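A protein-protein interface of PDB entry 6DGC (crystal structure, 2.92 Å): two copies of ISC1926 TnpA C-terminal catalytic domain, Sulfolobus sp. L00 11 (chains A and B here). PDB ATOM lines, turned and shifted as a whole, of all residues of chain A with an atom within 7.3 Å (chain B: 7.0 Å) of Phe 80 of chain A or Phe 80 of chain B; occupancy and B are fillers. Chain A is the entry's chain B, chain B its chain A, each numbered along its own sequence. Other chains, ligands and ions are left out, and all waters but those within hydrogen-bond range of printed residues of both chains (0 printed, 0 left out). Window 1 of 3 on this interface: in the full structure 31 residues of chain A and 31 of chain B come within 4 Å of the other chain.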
ATOM      1  N   GLY A  46       3.942  14.717  13.820  1.00  0.00           N
ATOM      2  CA  GLY A  46       2.540  14.334  13.623  1.00  0.00           C
ATOM      3  C   GLY A  46       1.841  15.165  12.540  1.00  0.00           C
ATOM      4  O   GLY A  46       0.848  14.735  11.951  1.00  0.00           O
ATOM      5  N   LEU A  47       2.386  16.363  12.267  1.00  0.00           N
ATOM      6  CA  LEU A  47       1.925  17.316  11.279  1.00  0.00           C
ATOM      7  C   LEU A  47       2.159  16.830   9.845  1.00  0.00           C
ATOM      8  O   LEU A  47       1.432  17.266   8.936  1.00  0.00           O
ATOM      9  CB  LEU A  47       2.639  18.677  11.478  1.00  0.00           C
ATOM     10  CG  LEU A  47       2.448  19.450  12.777  1.00  0.00           C
ATOM     11  CD1 LEU A  47       3.359  20.620  12.791  1.00  0.00           C
ATOM     12  CD2 LEU A  47       1.067  20.007  12.900  1.00  0.00           C
ATOM     13  N   THR A  49       1.616  14.686   6.953  1.00  0.00           N
ATOM     14  CA  THR A  49       0.607  13.779   6.393  1.00  0.00           C
ATOM     15  C   THR A  49       1.212  12.816   5.376  1.00  0.00           C
ATOM     16  O   THR A  49       0.502  11.932   4.884  1.00  0.00           O
ATOM     17  CB  THR A  49      -0.459  14.605   5.672  1.00  0.00           C
ATOM     18  OG1 THR A  49       0.198  15.596   4.878  1.00  0.00           O
ATOM     19  CG2 THR A  49      -1.418  15.256   6.624  1.00  0.00           C
ATOM     20  N   ARG A  51       4.131  10.887   5.823  1.00  0.00           N
ATOM     21  CA  ARG A  51       5.071   9.994   6.498  1.00  0.00           C
ATOM     22  C   ARG A  51       5.104   8.661   5.751  1.00  0.00           C
ATOM     23  O   ARG A  51       4.042   8.102   5.450  1.00  0.00           O
ATOM     24  CB  ARG A  51       4.659   9.782   7.964  1.00  0.00           C
ATOM     25  CG  ARG A  51       5.292  10.776   8.928  1.00  0.00           C
ATOM     26  CD  ARG A  51       4.667  10.761  10.310  1.00  0.00           C
ATOM     27  NE  ARG A  51       3.367  11.424  10.312  1.00  0.00           N
ATOM     28  CZ  ARG A  51       2.285  10.945  10.912  1.00  0.00           C
ATOM     29  NH1 ARG A  51       2.348   9.822  11.606  1.00  0.00           N
ATOM     30  NH2 ARG A  51       1.135  11.604  10.848  1.00  0.00           N
ATOM     31  N   ASP A  75      -2.149  11.173  19.399  1.00  0.00           N
ATOM     32  CA  ASP A  75      -1.016  12.068  19.050  1.00  0.00           C
ATOM     33  C   ASP A  75       0.003  11.398  18.118  1.00  0.00           C
ATOM     34  O   ASP A  75       0.519  12.055  17.223  1.00  0.00           O
ATOM     35  CB  ASP A  75      -0.275  12.536  20.331  1.00  0.00           C
ATOM     36  N   LEU A  77      -0.499   8.805  15.871  1.00  0.00           N
ATOM     37  CA  LEU A  77      -1.013   8.605  14.512  1.00  0.00           C
ATOM     38  C   LEU A  77      -0.954   9.865  13.689  1.00  0.00           C
ATOM     39  O   LEU A  77      -0.492   9.810  12.553  1.00  0.00           O
ATOM     40  CB  LEU A  77      -2.432   8.030  14.525  1.00  0.00           C
ATOM     41  CG  LEU A  77      -2.993   7.518  13.186  1.00  0.00           C
ATOM     42  CD1 LEU A  77      -2.082   6.489  12.539  1.00  0.00           C
ATOM     43  CD2 LEU A  77      -4.399   6.959  13.359  1.00  0.00           C
ATOM     44  N   THR A  78      -1.420  10.997  14.252  1.00  0.00           N
ATOM     45  CA  THR A  78      -1.446  12.312  13.589  1.00  0.00           C
ATOM     46  C   THR A  78      -1.746  13.446  14.585  1.00  0.00           C
ATOM     47  O   THR A  78      -2.562  13.250  15.499  1.00  0.00           O
ATOM     48  CB  THR A  78      -2.416  12.329  12.382  1.00  0.00           C
ATOM     49  OG1 THR A  78      -2.349  13.603  11.750  1.00  0.00           O
ATOM     50  CG2 THR A  78      -3.847  12.004  12.755  1.00  0.00           C
ATOM     51  N   ARG A  79      -1.102  14.626  14.394  1.00  0.00           N
ATOM     52  CA  ARG A  79      -1.337  15.811  15.217  1.00  0.00           C
ATOM     53  C   ARG A  79      -2.749  16.334  14.967  1.00  0.00           C
ATOM     54  O   ARG A  79      -3.442  16.652  15.930  1.00  0.00           O
ATOM     55  CB  ARG A  79      -0.294  16.906  14.937  1.00  0.00           C
ATOM     56  CG  ARG A  79      -0.553  18.247  15.643  1.00  0.00           C
ATOM     57  CD  ARG A  79      -0.576  18.174  17.150  1.00  0.00           C
ATOM     58  NE  ARG A  79       0.742  17.852  17.689  1.00  0.00           N
ATOM     59  CZ  ARG A  79       0.942  17.294  18.874  1.00  0.00           C
ATOM     60  NH1 ARG A  79      -0.084  17.029  19.674  1.00  0.00           N
ATOM     61  NH2 ARG A  79       2.170  16.998  19.272  1.00  0.00           N
ATOM     62  N   PHE A  80      -3.158  16.435  13.672  1.00  0.00           N
ATOM     63  CA  PHE A  80      -4.483  16.909  13.264  1.00  0.00           C
ATOM     64  C   PHE A  80      -5.168  15.939  12.310  1.00  0.00           C
ATOM     65  O   PHE A  80      -4.493  15.179  11.614  1.00  0.00           O
ATOM     66  CB  PHE A  80      -4.394  18.276  12.587  1.00  0.00           C
ATOM     67  CG  PHE A  80      -3.863  19.421  13.412  1.00  0.00           C
ATOM     68  CD1 PHE A  80      -4.578  19.912  14.497  1.00  0.00           C
ATOM     69  CD2 PHE A  80      -2.703  20.077  13.043  1.00  0.00           C
ATOM     70  CE1 PHE A  80      -4.109  20.997  15.227  1.00  0.00           C
ATOM     71  CE2 PHE A  80      -2.244  21.171  13.767  1.00  0.00           C
ATOM     72  CZ  PHE A  80      -2.942  21.617  14.859  1.00  0.00           C
ATOM     73  N   GLY A  81      -6.497  16.001  12.261  1.00  0.00           N
ATOM     74  CA  GLY A  81      -7.304  15.179  11.363  1.00  0.00           C
ATOM     75  C   GLY A  81      -7.353  13.696  11.652  1.00  0.00           C
ATOM     76  O   GLY A  81      -7.499  12.897  10.717  1.00  0.00           O
ATOM     77  N   PHE A  82      -7.273  13.317  12.934  1.00  0.00           N
ATOM     78  CA  PHE A  82      -7.374  11.919  13.362  1.00  0.00           C
ATOM     79  C   PHE A  82      -8.677  11.331  12.827  1.00  0.00           C
ATOM     80  O   PHE A  82      -8.668  10.283  12.185  1.00  0.00           O
ATOM     81  CB  PHE A  82      -7.351  11.833  14.896  1.00  0.00           C
ATOM     82  CG  PHE A  82      -7.444  10.449  15.469  1.00  0.00           C
ATOM     83  CD1 PHE A  82      -8.677   9.890  15.784  1.00  0.00           C
ATOM     84  CD2 PHE A  82      -6.292   9.697  15.706  1.00  0.00           C
ATOM     85  CE1 PHE A  82      -8.756   8.590  16.305  1.00  0.00           C
ATOM     86  CE2 PHE A  82      -6.373   8.395  16.220  1.00  0.00           C
ATOM     87  CZ  PHE A  82      -7.604   7.853  16.516  1.00  0.00           C
ATOM     88  N   GLU A  83      -9.779  12.078  12.998  1.00  0.00           N
ATOM     89  CA  GLU A  83     -11.139  11.692  12.634  1.00  0.00           C
ATOM     90  C   GLU A  83     -11.275  11.252  11.180  1.00  0.00           C
ATOM     91  O   GLU A  83     -12.048  10.322  10.903  1.00  0.00           O
ATOM     92  CB  GLU A  83     -12.144  12.796  13.006  1.00  0.00           C
ATOM     93  CG  GLU A  83     -12.175  13.142  14.498  1.00  0.00           C
ATOM     94  CD  GLU A  83     -12.391  11.993  15.479  1.00  0.00           C
ATOM     95  OE1 GLU A  83     -13.459  11.341  15.396  1.00  0.00           O
ATOM     96  OE2 GLU A  83     -11.494  11.741  16.323  1.00  0.00           O
ATOM     97  N   TYR A  84     -10.474  11.862  10.268  1.00  0.00           N
ATOM     98  CA  TYR A  84     -10.463  11.515   8.840  1.00  0.00           C
ATOM     99  C   TYR A  84      -9.793  10.155   8.658  1.00  0.00           C
ATOM    100  O   TYR A  84     -10.311   9.320   7.898  1.00  0.00           O
ATOM    101  CB  TYR A  84      -9.734  12.573   7.998  1.00  0.00           C
ATOM    102  CG  TYR A  84     -10.173  14.007   8.210  1.00  0.00           C
ATOM    103  CD1 TYR A  84     -11.520  14.337   8.306  1.00  0.00           C
ATOM    104  CD2 TYR A  84      -9.248  15.043   8.200  1.00  0.00           C
ATOM    105  CE1 TYR A  84     -11.929  15.655   8.458  1.00  0.00           C
ATOM    106  CE2 TYR A  84      -9.648  16.368   8.323  1.00  0.00           C
ATOM    107  CZ  TYR A  84     -10.989  16.667   8.464  1.00  0.00           C
ATOM    108  OH  TYR A  84     -11.395  17.964   8.628  1.00  0.00           O
ATOM    109  N   ILE A  85      -8.654   9.925   9.381  1.00  0.00           N
ATOM    110  CA  ILE A  85      -7.936   8.642   9.326  1.00  0.00           C
ATOM    111  C   ILE A  85      -8.835   7.545   9.882  1.00  0.00           C
ATOM    112  O   ILE A  85      -8.958   6.476   9.267  1.00  0.00           O
ATOM    113  CB  ILE A  85      -6.546   8.658  10.004  1.00  0.00           C
ATOM    114  CG1 ILE A  85      -5.664   9.808   9.466  1.00  0.00           C
ATOM    115  CG2 ILE A  85      -5.857   7.317   9.797  1.00  0.00           C
ATOM    116  CD1 ILE A  85      -4.255   9.858  10.048  1.00  0.00           C
ATOM    117  N   ASP A 114       5.794  21.717  17.619  1.00  0.00           N
ATOM    118  CA  ASP A 114       4.730  21.635  16.622  1.00  0.00           C
ATOM    119  C   ASP A 114       3.970  22.951  16.522  1.00  0.00           C
ATOM    120  O   ASP A 114       3.563  23.320  15.420  1.00  0.00           O
ATOM    121  CB  ASP A 114       3.765  20.467  16.909  1.00  0.00           C
ATOM    122  CG  ASP A 114       4.159  19.103  16.339  1.00  0.00           C
ATOM    123  OD1 ASP A 114       5.157  19.035  15.576  1.00  0.00           O
ATOM    124  OD2 ASP A 114       3.462  18.103  16.649  1.00  0.00           O
ATOM    125  N   ILE A 118       3.653  25.491  13.037  1.00  0.00           N
ATOM    126  CA  ILE A 118       2.303  25.883  12.584  1.00  0.00           C
ATOM    127  C   ILE A 118       2.286  27.429  12.438  1.00  0.00           C
ATOM    128  O   ILE A 118       1.897  27.949  11.381  1.00  0.00           O
ATOM    129  CB  ILE A 118       1.180  25.364  13.551  1.00  0.00           C
ATOM    130  CG1 ILE A 118       1.084  23.833  13.585  1.00  0.00           C
ATOM    131  CG2 ILE A 118      -0.186  25.968  13.229  1.00  0.00           C
ATOM    132  CD1 ILE A 118       0.477  23.265  14.914  1.00  0.00           C
ATOM    133  N   SER A 121       4.355  28.636   9.418  1.00  0.00           N
ATOM    134  CA  SER A 121       3.659  28.430   8.138  1.00  0.00           C
ATOM    135  C   SER A 121       2.509  29.443   7.957  1.00  0.00           C
ATOM    136  O   SER A 121       2.474  30.156   6.947  1.00  0.00           O
ATOM    137  CB  SER A 121       3.160  27.001   8.016  1.00  0.00           C
ATOM    138  OG  SER A 121       2.040  26.811   8.862  1.00  0.00           O
ATOM    139  N   PHE A 122       1.619  29.540   8.977  1.00  0.00           N
ATOM    140  CA  PHE A 122       0.489  30.475   9.021  1.00  0.00           C
ATOM    141  C   PHE A 122       0.956  31.923   8.902  1.00  0.00           C
ATOM    142  O   PHE A 122       0.318  32.668   8.166  1.00  0.00           O
ATOM    143  CB  PHE A 122      -0.296  30.299  10.319  1.00  0.00           C
ATOM    144  CG  PHE A 122      -1.506  29.413  10.254  1.00  0.00           C
ATOM    145  CD1 PHE A 122      -1.378  28.032  10.307  1.00  0.00           C
ATOM    146  CD2 PHE A 122      -2.780  29.959  10.250  1.00  0.00           C
ATOM    147  CE1 PHE A 122      -2.506  27.210  10.292  1.00  0.00           C
ATOM    148  CE2 PHE A 122      -3.906  29.140  10.245  1.00  0.00           C
ATOM    149  CZ  PHE A 122      -3.762  27.771  10.256  1.00  0.00           C
ATOM    150  N   GLY B  46     -12.674  25.460   9.275  1.00  0.00           N
ATOM    151  CA  GLY B  46     -12.021  24.334   8.605  1.00  0.00           C
ATOM    152  C   GLY B  46     -11.414  23.355   9.594  1.00  0.00           C
ATOM    153  O   GLY B  46     -11.211  22.177   9.275  1.00  0.00           O
ATOM    154  N   LEU B  47     -11.144  23.854  10.825  1.00  0.00           N
ATOM    155  CA  LEU B  47     -10.588  23.122  11.965  1.00  0.00           C
ATOM    156  C   LEU B  47     -11.595  22.117  12.563  1.00  0.00           C
ATOM    157  O   LEU B  47     -11.172  21.182  13.239  1.00  0.00           O
ATOM    158  CB  LEU B  47     -10.114  24.104  13.058  1.00  0.00           C
ATOM    159  CG  LEU B  47      -8.997  25.123  12.737  1.00  0.00           C
ATOM    160  CD1 LEU B  47      -8.858  26.102  13.844  1.00  0.00           C
ATOM    161  CD2 LEU B  47      -7.654  24.480  12.606  1.00  0.00           C
ATOM    162  N   THR B  49     -13.553  19.051  12.416  1.00  0.00           N
ATOM    163  CA  THR B  49     -13.585  17.755  11.720  1.00  0.00           C
ATOM    164  C   THR B  49     -14.978  17.108  11.755  1.00  0.00           C
ATOM    165  O   THR B  49     -15.198  16.085  11.096  1.00  0.00           O
ATOM    166  CB  THR B  49     -12.582  16.804  12.382  1.00  0.00           C
ATOM    167  OG1 THR B  49     -12.764  16.895  13.793  1.00  0.00           O
ATOM    168  CG2 THR B  49     -11.143  17.131  12.029  1.00  0.00           C
ATOM    169  N   ARG B  51     -18.070  18.733  11.087  1.00  0.00           N
ATOM    170  CA  ARG B  51     -19.039  19.582  10.387  1.00  0.00           C
ATOM    171  C   ARG B  51     -20.147  18.711   9.823  1.00  0.00           C
ATOM    172  O   ARG B  51     -19.857  17.706   9.173  1.00  0.00           O
ATOM    173  CB  ARG B  51     -18.362  20.364   9.253  1.00  0.00           C
ATOM    174  CG  ARG B  51     -17.870  21.749   9.658  1.00  0.00           C
ATOM    175  CD  ARG B  51     -16.928  22.348   8.628  1.00  0.00           C
ATOM    176  NE  ARG B  51     -15.616  21.687   8.654  1.00  0.00           N
ATOM    177  CZ  ARG B  51     -14.944  21.309   7.571  1.00  0.00           C
ATOM    178  NH1 ARG B  51     -15.426  21.552   6.366  1.00  0.00           N
ATOM    179  NH2 ARG B  51     -13.771  20.701   7.689  1.00  0.00           N
ATOM    180  N   ASP B  75      -8.622  24.706   1.187  1.00  0.00           N
ATOM    181  CA  ASP B  75      -8.944  25.429   2.426  1.00  0.00           C
ATOM    182  C   ASP B  75     -10.414  25.195   2.893  1.00  0.00           C
ATOM    183  O   ASP B  75     -10.646  24.951   4.086  1.00  0.00           O
ATOM    184  CB  ASP B  75      -8.694  26.942   2.163  1.00  0.00           C
ATOM    185  CG  ASP B  75      -8.648  27.818   3.397  1.00  0.00           C
ATOM    186  OD1 ASP B  75      -8.594  27.259   4.529  1.00  0.00           O
ATOM    187  OD2 ASP B  75      -8.625  29.063   3.239  1.00  0.00           O
ATOM    188  N   LEU B  77     -12.506  22.612   2.132  1.00  0.00           N
ATOM    189  CA  LEU B  77     -12.791  21.250   2.577  1.00  0.00           C
ATOM    190  C   LEU B  77     -12.360  21.030   4.015  1.00  0.00           C
ATOM    191  O   LEU B  77     -13.127  20.468   4.792  1.00  0.00           O
ATOM    192  CB  LEU B  77     -12.157  20.215   1.640  1.00  0.00           C
ATOM    193  CG  LEU B  77     -12.573  18.763   1.829  1.00  0.00           C
ATOM    194  CD1 LEU B  77     -14.081  18.606   1.769  1.00  0.00           C
ATOM    195  CD2 LEU B  77     -11.897  17.874   0.799  1.00  0.00           C
ATOM    196  N   THR B  78     -11.140  21.473   4.370  1.00  0.00           N
ATOM    197  CA  THR B  78     -10.550  21.306   5.702  1.00  0.00           C
ATOM    198  C   THR B  78      -9.288  22.143   5.866  1.00  0.00           C
ATOM    199  O   THR B  78      -8.525  22.284   4.903  1.00  0.00           O
ATOM    200  CB  THR B  78     -10.274  19.813   6.024  1.00  0.00           C
ATOM    201  OG1 THR B  78      -9.760  19.705   7.356  1.00  0.00           O
ATOM    202  CG2 THR B  78      -9.333  19.125   5.024  1.00  0.00           C
ATOM    203  N   ARG B  79      -9.051  22.680   7.093  1.00  0.00           N
ATOM    204  CA  ARG B  79      -7.846  23.449   7.398  1.00  0.00           C
ATOM    205  C   ARG B  79      -6.635  22.525   7.400  1.00  0.00           C
ATOM    206  O   ARG B  79      -5.616  22.869   6.787  1.00  0.00           O
ATOM    207  CB  ARG B  79      -7.961  24.204   8.723  1.00  0.00           C
ATOM    208  CG  ARG B  79      -6.664  24.917   9.141  1.00  0.00           C
ATOM    209  CD  ARG B  79      -6.151  25.966   8.150  1.00  0.00           C
ATOM    210  NE  ARG B  79      -7.079  27.092   8.050  1.00  0.00           N
ATOM    211  CZ  ARG B  79      -7.114  27.938   7.033  1.00  0.00           C
ATOM    212  NH1 ARG B  79      -6.262  27.809   6.025  1.00  0.00           N
ATOM    213  NH2 ARG B  79      -8.017  28.908   7.002  1.00  0.00           N
ATOM    214  N   PHE B  80      -6.754  21.359   8.075  1.00  0.00           N
ATOM    215  CA  PHE B  80      -5.675  20.365   8.148  1.00  0.00           C
ATOM    216  C   PHE B  80      -6.127  18.988   7.695  1.00  0.00           C
ATOM    217  O   PHE B  80      -7.315  18.668   7.779  1.00  0.00           O
ATOM    218  CB  PHE B  80      -5.082  20.262   9.570  1.00  0.00           C
ATOM    219  CG  PHE B  80      -4.434  21.503  10.117  1.00  0.00           C
ATOM    220  CD1 PHE B  80      -3.265  21.996   9.561  1.00  0.00           C
ATOM    221  CD2 PHE B  80      -4.956  22.144  11.226  1.00  0.00           C
ATOM    222  CE1 PHE B  80      -2.657  23.146  10.067  1.00  0.00           C
ATOM    223  CE2 PHE B  80      -4.345  23.286  11.741  1.00  0.00           C
ATOM    224  CZ  PHE B  80      -3.202  23.789  11.153  1.00  0.00           C
ATOM    225  N   GLY B  81      -5.168  18.181   7.257  1.00  0.00           N
ATOM    226  CA  GLY B  81      -5.431  16.811   6.852  1.00  0.00           C
ATOM    227  C   GLY B  81      -6.226  16.600   5.584  1.00  0.00           C
ATOM    228  O   GLY B  81      -6.955  15.609   5.494  1.00  0.00           O
ATOM    229  N   PHE B  82      -6.049  17.479   4.572  1.00  0.00           N
ATOM    230  CA  PHE B  82      -6.707  17.346   3.268  1.00  0.00           C
ATOM    231  C   PHE B  82      -6.334  16.016   2.634  1.00  0.00           C
ATOM    232  O   PHE B  82      -7.180  15.366   2.041  1.00  0.00           O
ATOM    233  CB  PHE B  82      -6.300  18.493   2.325  1.00  0.00           C
ATOM    234  CG  PHE B  82      -6.992  18.513   0.969  1.00  0.00           C
ATOM    235  CD1 PHE B  82      -6.484  17.781  -0.105  1.00  0.00           C
ATOM    236  CD2 PHE B  82      -8.130  19.287   0.761  1.00  0.00           C
ATOM    237  CE1 PHE B  82      -7.134  17.781  -1.343  1.00  0.00           C
ATOM    238  CE2 PHE B  82      -8.787  19.276  -0.475  1.00  0.00           C
ATOM    239  CZ  PHE B  82      -8.282  18.521  -1.517  1.00  0.00           C
ATOM    240  N   GLU B  83      -5.075  15.615   2.784  1.00  0.00           N
ATOM    241  CA  GLU B  83      -4.480  14.403   2.221  1.00  0.00           C
ATOM    242  C   GLU B  83      -5.180  13.143   2.681  1.00  0.00           C
ATOM    243  O   GLU B  83      -5.305  12.203   1.883  1.00  0.00           O
ATOM    244  CB  GLU B  83      -2.956  14.370   2.495  1.00  0.00           C
ATOM    245  CG  GLU B  83      -2.170  15.563   1.925  1.00  0.00           C
ATOM    246  CD  GLU B  83      -2.329  15.777   0.424  1.00  0.00           C
ATOM    247  OE1 GLU B  83      -2.032  14.836  -0.350  1.00  0.00           O
ATOM    248  OE2 GLU B  83      -2.791  16.873   0.024  1.00  0.00           O
ATOM    249  N   TYR B  84      -5.685  13.143   3.946  1.00  0.00           N
ATOM    250  CA  TYR B  84      -6.433  12.015   4.526  1.00  0.00           C
ATOM    251  C   TYR B  84      -7.809  11.934   3.864  1.00  0.00           C
ATOM    252  O   TYR B  84      -8.242  10.842   3.489  1.00  0.00           O
ATOM    253  CB  TYR B  84      -6.584  12.145   6.054  1.00  0.00           C
ATOM    254  CG  TYR B  84      -5.299  12.396   6.823  1.00  0.00           C
ATOM    255  CD1 TYR B  84      -4.135  11.692   6.528  1.00  0.00           C
ATOM    256  CD2 TYR B  84      -5.274  13.258   7.916  1.00  0.00           C
ATOM    257  CE1 TYR B  84      -2.958  11.899   7.252  1.00  0.00           C
ATOM    258  CE2 TYR B  84      -4.101  13.473   8.648  1.00  0.00           C
ATOM    259  CZ  TYR B  84      -2.944  12.790   8.313  1.00  0.00           C
ATOM    260  OH  TYR B  84      -1.765  13.013   8.996  1.00  0.00           O
ATOM    261  N   ILE B  85      -8.478  13.104   3.683  1.00  0.00           N
ATOM    262  CA  ILE B  85      -9.799  13.175   3.034  1.00  0.00           C
ATOM    263  C   ILE B  85      -9.653  12.715   1.593  1.00  0.00           C
ATOM    264  O   ILE B  85     -10.446  11.888   1.143  1.00  0.00           O
ATOM    265  CB  ILE B  85     -10.514  14.537   3.165  1.00  0.00           C
ATOM    266  CG1 ILE B  85     -10.604  14.986   4.619  1.00  0.00           C
ATOM    267  CG2 ILE B  85     -11.907  14.443   2.566  1.00  0.00           C
ATOM    268  CD1 ILE B  85     -11.327  16.285   4.837  1.00  0.00           C
ATOM    269  N   ASP B 114      -8.300  31.183  12.810  1.00  0.00           N
ATOM    270  CA  ASP B 114      -7.898  29.788  12.964  1.00  0.00           C
ATOM    271  C   ASP B 114      -6.617  29.681  13.733  1.00  0.00           C
ATOM    272  O   ASP B 114      -6.503  28.791  14.563  1.00  0.00           O
ATOM    273  CB  ASP B 114      -7.775  29.078  11.613  1.00  0.00           C
ATOM    274  CG  ASP B 114      -9.099  28.535  11.088  1.00  0.00           C
ATOM    275  OD1 ASP B 114     -10.104  28.571  11.849  1.00  0.00           O
ATOM    276  OD2 ASP B 114      -9.134  28.065   9.917  1.00  0.00           O
ATOM    277  N   ILE B 118      -5.923  27.634  17.375  1.00  0.00           N
ATOM    278  CA  ILE B 118      -4.839  26.640  17.426  1.00  0.00           C
ATOM    279  C   ILE B 118      -3.946  26.929  18.667  1.00  0.00           C
ATOM    280  O   ILE B 118      -3.748  26.043  19.507  1.00  0.00           O
ATOM    281  CB  ILE B 118      -4.032  26.552  16.080  1.00  0.00           C
ATOM    282  CG1 ILE B 118      -4.907  26.061  14.914  1.00  0.00           C
ATOM    283  CG2 ILE B 118      -2.780  25.657  16.227  1.00  0.00           C
ATOM    284  CD1 ILE B 118      -4.389  26.483  13.516  1.00  0.00           C
ATOM    285  N   SER B 121      -5.854  26.197  21.955  1.00  0.00           N
ATOM    286  CA  SER B 121      -5.935  24.771  22.244  1.00  0.00           C
ATOM    287  C   SER B 121      -4.569  24.232  22.714  1.00  0.00           C
ATOM    288  O   SER B 121      -4.498  23.612  23.783  1.00  0.00           O
ATOM    289  CB  SER B 121      -6.444  23.997  21.037  1.00  0.00           C
ATOM    290  OG  SER B 121      -5.437  23.893  20.045  1.00  0.00           O
ATOM    291  N   PHE B 122      -3.488  24.517  21.938  1.00  0.00           N
ATOM    292  CA  PHE B 122      -2.107  24.128  22.239  1.00  0.00           C
ATOM    293  C   PHE B 122      -1.651  24.679  23.594  1.00  0.00           C
ATOM    294  O   PHE B 122      -1.003  23.945  24.335  1.00  0.00           O
ATOM    295  CB  PHE B 122      -1.156  24.598  21.139  1.00  0.00           C
ATOM    296  CG  PHE B 122      -0.829  23.571  20.088  1.00  0.00           C
ATOM    297  CD1 PHE B 122      -1.713  23.314  19.039  1.00  0.00           C
ATOM    298  CD2 PHE B 122       0.382  22.890  20.113  1.00  0.00           C
ATOM    299  CE1 PHE B 122      -1.409  22.360  18.049  1.00  0.00           C
ATOM    300  CE2 PHE B 122       0.688  21.944  19.119  1.00  0.00           C
ATOM    301  CZ  PHE B 122      -0.209  21.690  18.090  1.00  0.00           C
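The side-chain hydroxyl of Thr 78 of chain B is in hydrogen-bond range of the side-chain hydroxyl of Tyr 84 of chain A, at 2.7 Å.
OH of Tyr 84 of chain B lies within hydrogen-bond range of OG1 of Thr 78 of chain A, at 2.9 Å.
The side-chain carboxylate of Asp 75 of chain B lies within salt-bridge range of the guanidinium group of Arg 79 of chain B (2.8 Å).
NE of Arg 79 of chain B is in salt-bridge range of OD2 of Asp 114 of chain B (2.9 Å).
OG1 of Thr 78 of chain A sits at hydrogen-bond distance from O of Gly 46 of chain A (3.4 Å).
NH2 of Arg 51 of chain A is in hydrogen-bond range of O of Leu 77 of chain A (3.0 Å).
Among the printed residues, pairs that only touch across the chains: Thr 49 of chain A with Glu 83 of chain B (3.8 Å), Thr 49 of chain A with Tyr 84 of chain B (3.3 Å), Arg 51 of chain A with Tyr 84 of chain B (3.7 Å), Arg 79 of chain A with Phe 122 of chain B (3.7 Å), Phe 80 of chain A with Phe 80 of chain B (3.6 Å), Phe 80 of chain A with Tyr 84 of chain B (3.4 Å), Phe 80 of chain A with Phe 122 of chain B (3.6 Å), Gly 81 of chain A with Tyr 84 of chain B (3.6 Å), Glu 83 of chain A with Thr 49 of chain B (3.9 Å), Tyr 84 of chain A with Thr 49 of chain B (3.5 Å), Tyr 84 of chain A with Arg 51 of chain B (3.7 Å), Tyr 84 of chain A with Phe 80 of chain B (3.3 Å), Tyr 84 of chain A with Gly 81 of chain B (3.6 Å), Tyr 84 of chain A with Tyr 84 of chain B (3.7 Å), Tyr 84 of chain A with Ile 85 of chain B (3.7 Å), Ile 85 of chain A with Tyr 84 of chain B (3.7 Å), Ile 118 of chain A with Ile 118 of chain B (3.98 Å), Ile 118 of chain A with Phe 122 of chain B (3.6 Å), Phe 122 of chain A with Arg 79 of chain B (3.7 Å), Phe 122 of chain A with Phe 80 of chain B (3.6 Å) and Phe 122 of chain A with Ile 118 of chain B (3.6 Å).
Phe 80 of chain A touches just these residues of chain B: Phe 80, Tyr 84 and Phe 122.
Of chain A, only Phe 80 (3.6 Å), Tyr 84 (3.3 Å) and Phe 122 (3.6 Å) come within 4 Å of Phe 80 of chain B.
Of the printed residues of chain A, Ile 118 of chain B touches Ile 118 (3.98 Å) and Phe 122 (3.6 Å).
Of the printed residues of chain A, Gly 81 of chain B touches Tyr 84 (3.6 Å).
Of the printed residues of chain B, Arg 79 of chain A touches Phe 122 (3.7 Å).
Of the printed residues of chain A, Thr 49 of chain B touches Glu 83 and Tyr 84.
Leu 47 of chain A touches none of the printed residues of chain B.
Ser 121 of chain B touches none of the printed residues of chain A.
The nearest residue of chain A that does not touch Phe 80 of chain B is Ile 118 of chain A (4.3 Å).
Of the 18 printed residues of chain A, 11 touch a printed residue of chain B.
Hydrophobic or aromatic side chains of chain A within 4 Å of the printed part of chain B: Phe 80, Tyr 84, Ile 85, Ile 118 and Phe 122.
Of the 18 printed residues of chain B, 11 touch a printed residue of chain A.
Printed residues of chain B that touch a printed residue of chain A: Thr 49, Arg 51, Thr 78, Arg 79, Phe 80, Gly 81, Glu 83, Tyr 84, Ile 85, Ile 118 and Phe 122.
Among the printed residues, no Asp or Glu carboxylate lies within 4 Å of a Lys or Arg side-chain nitrogen of the other chain.
Arg 51 of chain A touches Tyr 84 of chain B, and with the chains exchanged Tyr 84 of chain A touches Arg 51 of chain B.
Phe 80 of chain A touches Phe 122 of chain B, and with the chains exchanged Phe 122 of chain A touches Phe 80 of chain B.
Gly 81 of chain A touches Tyr 84 of chain B, and with the chains exchanged Tyr 84 of chain A touches Gly 81 of chain B.
Tyr 84 of chain B touches its own counterpart, Tyr 84 of chain A.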
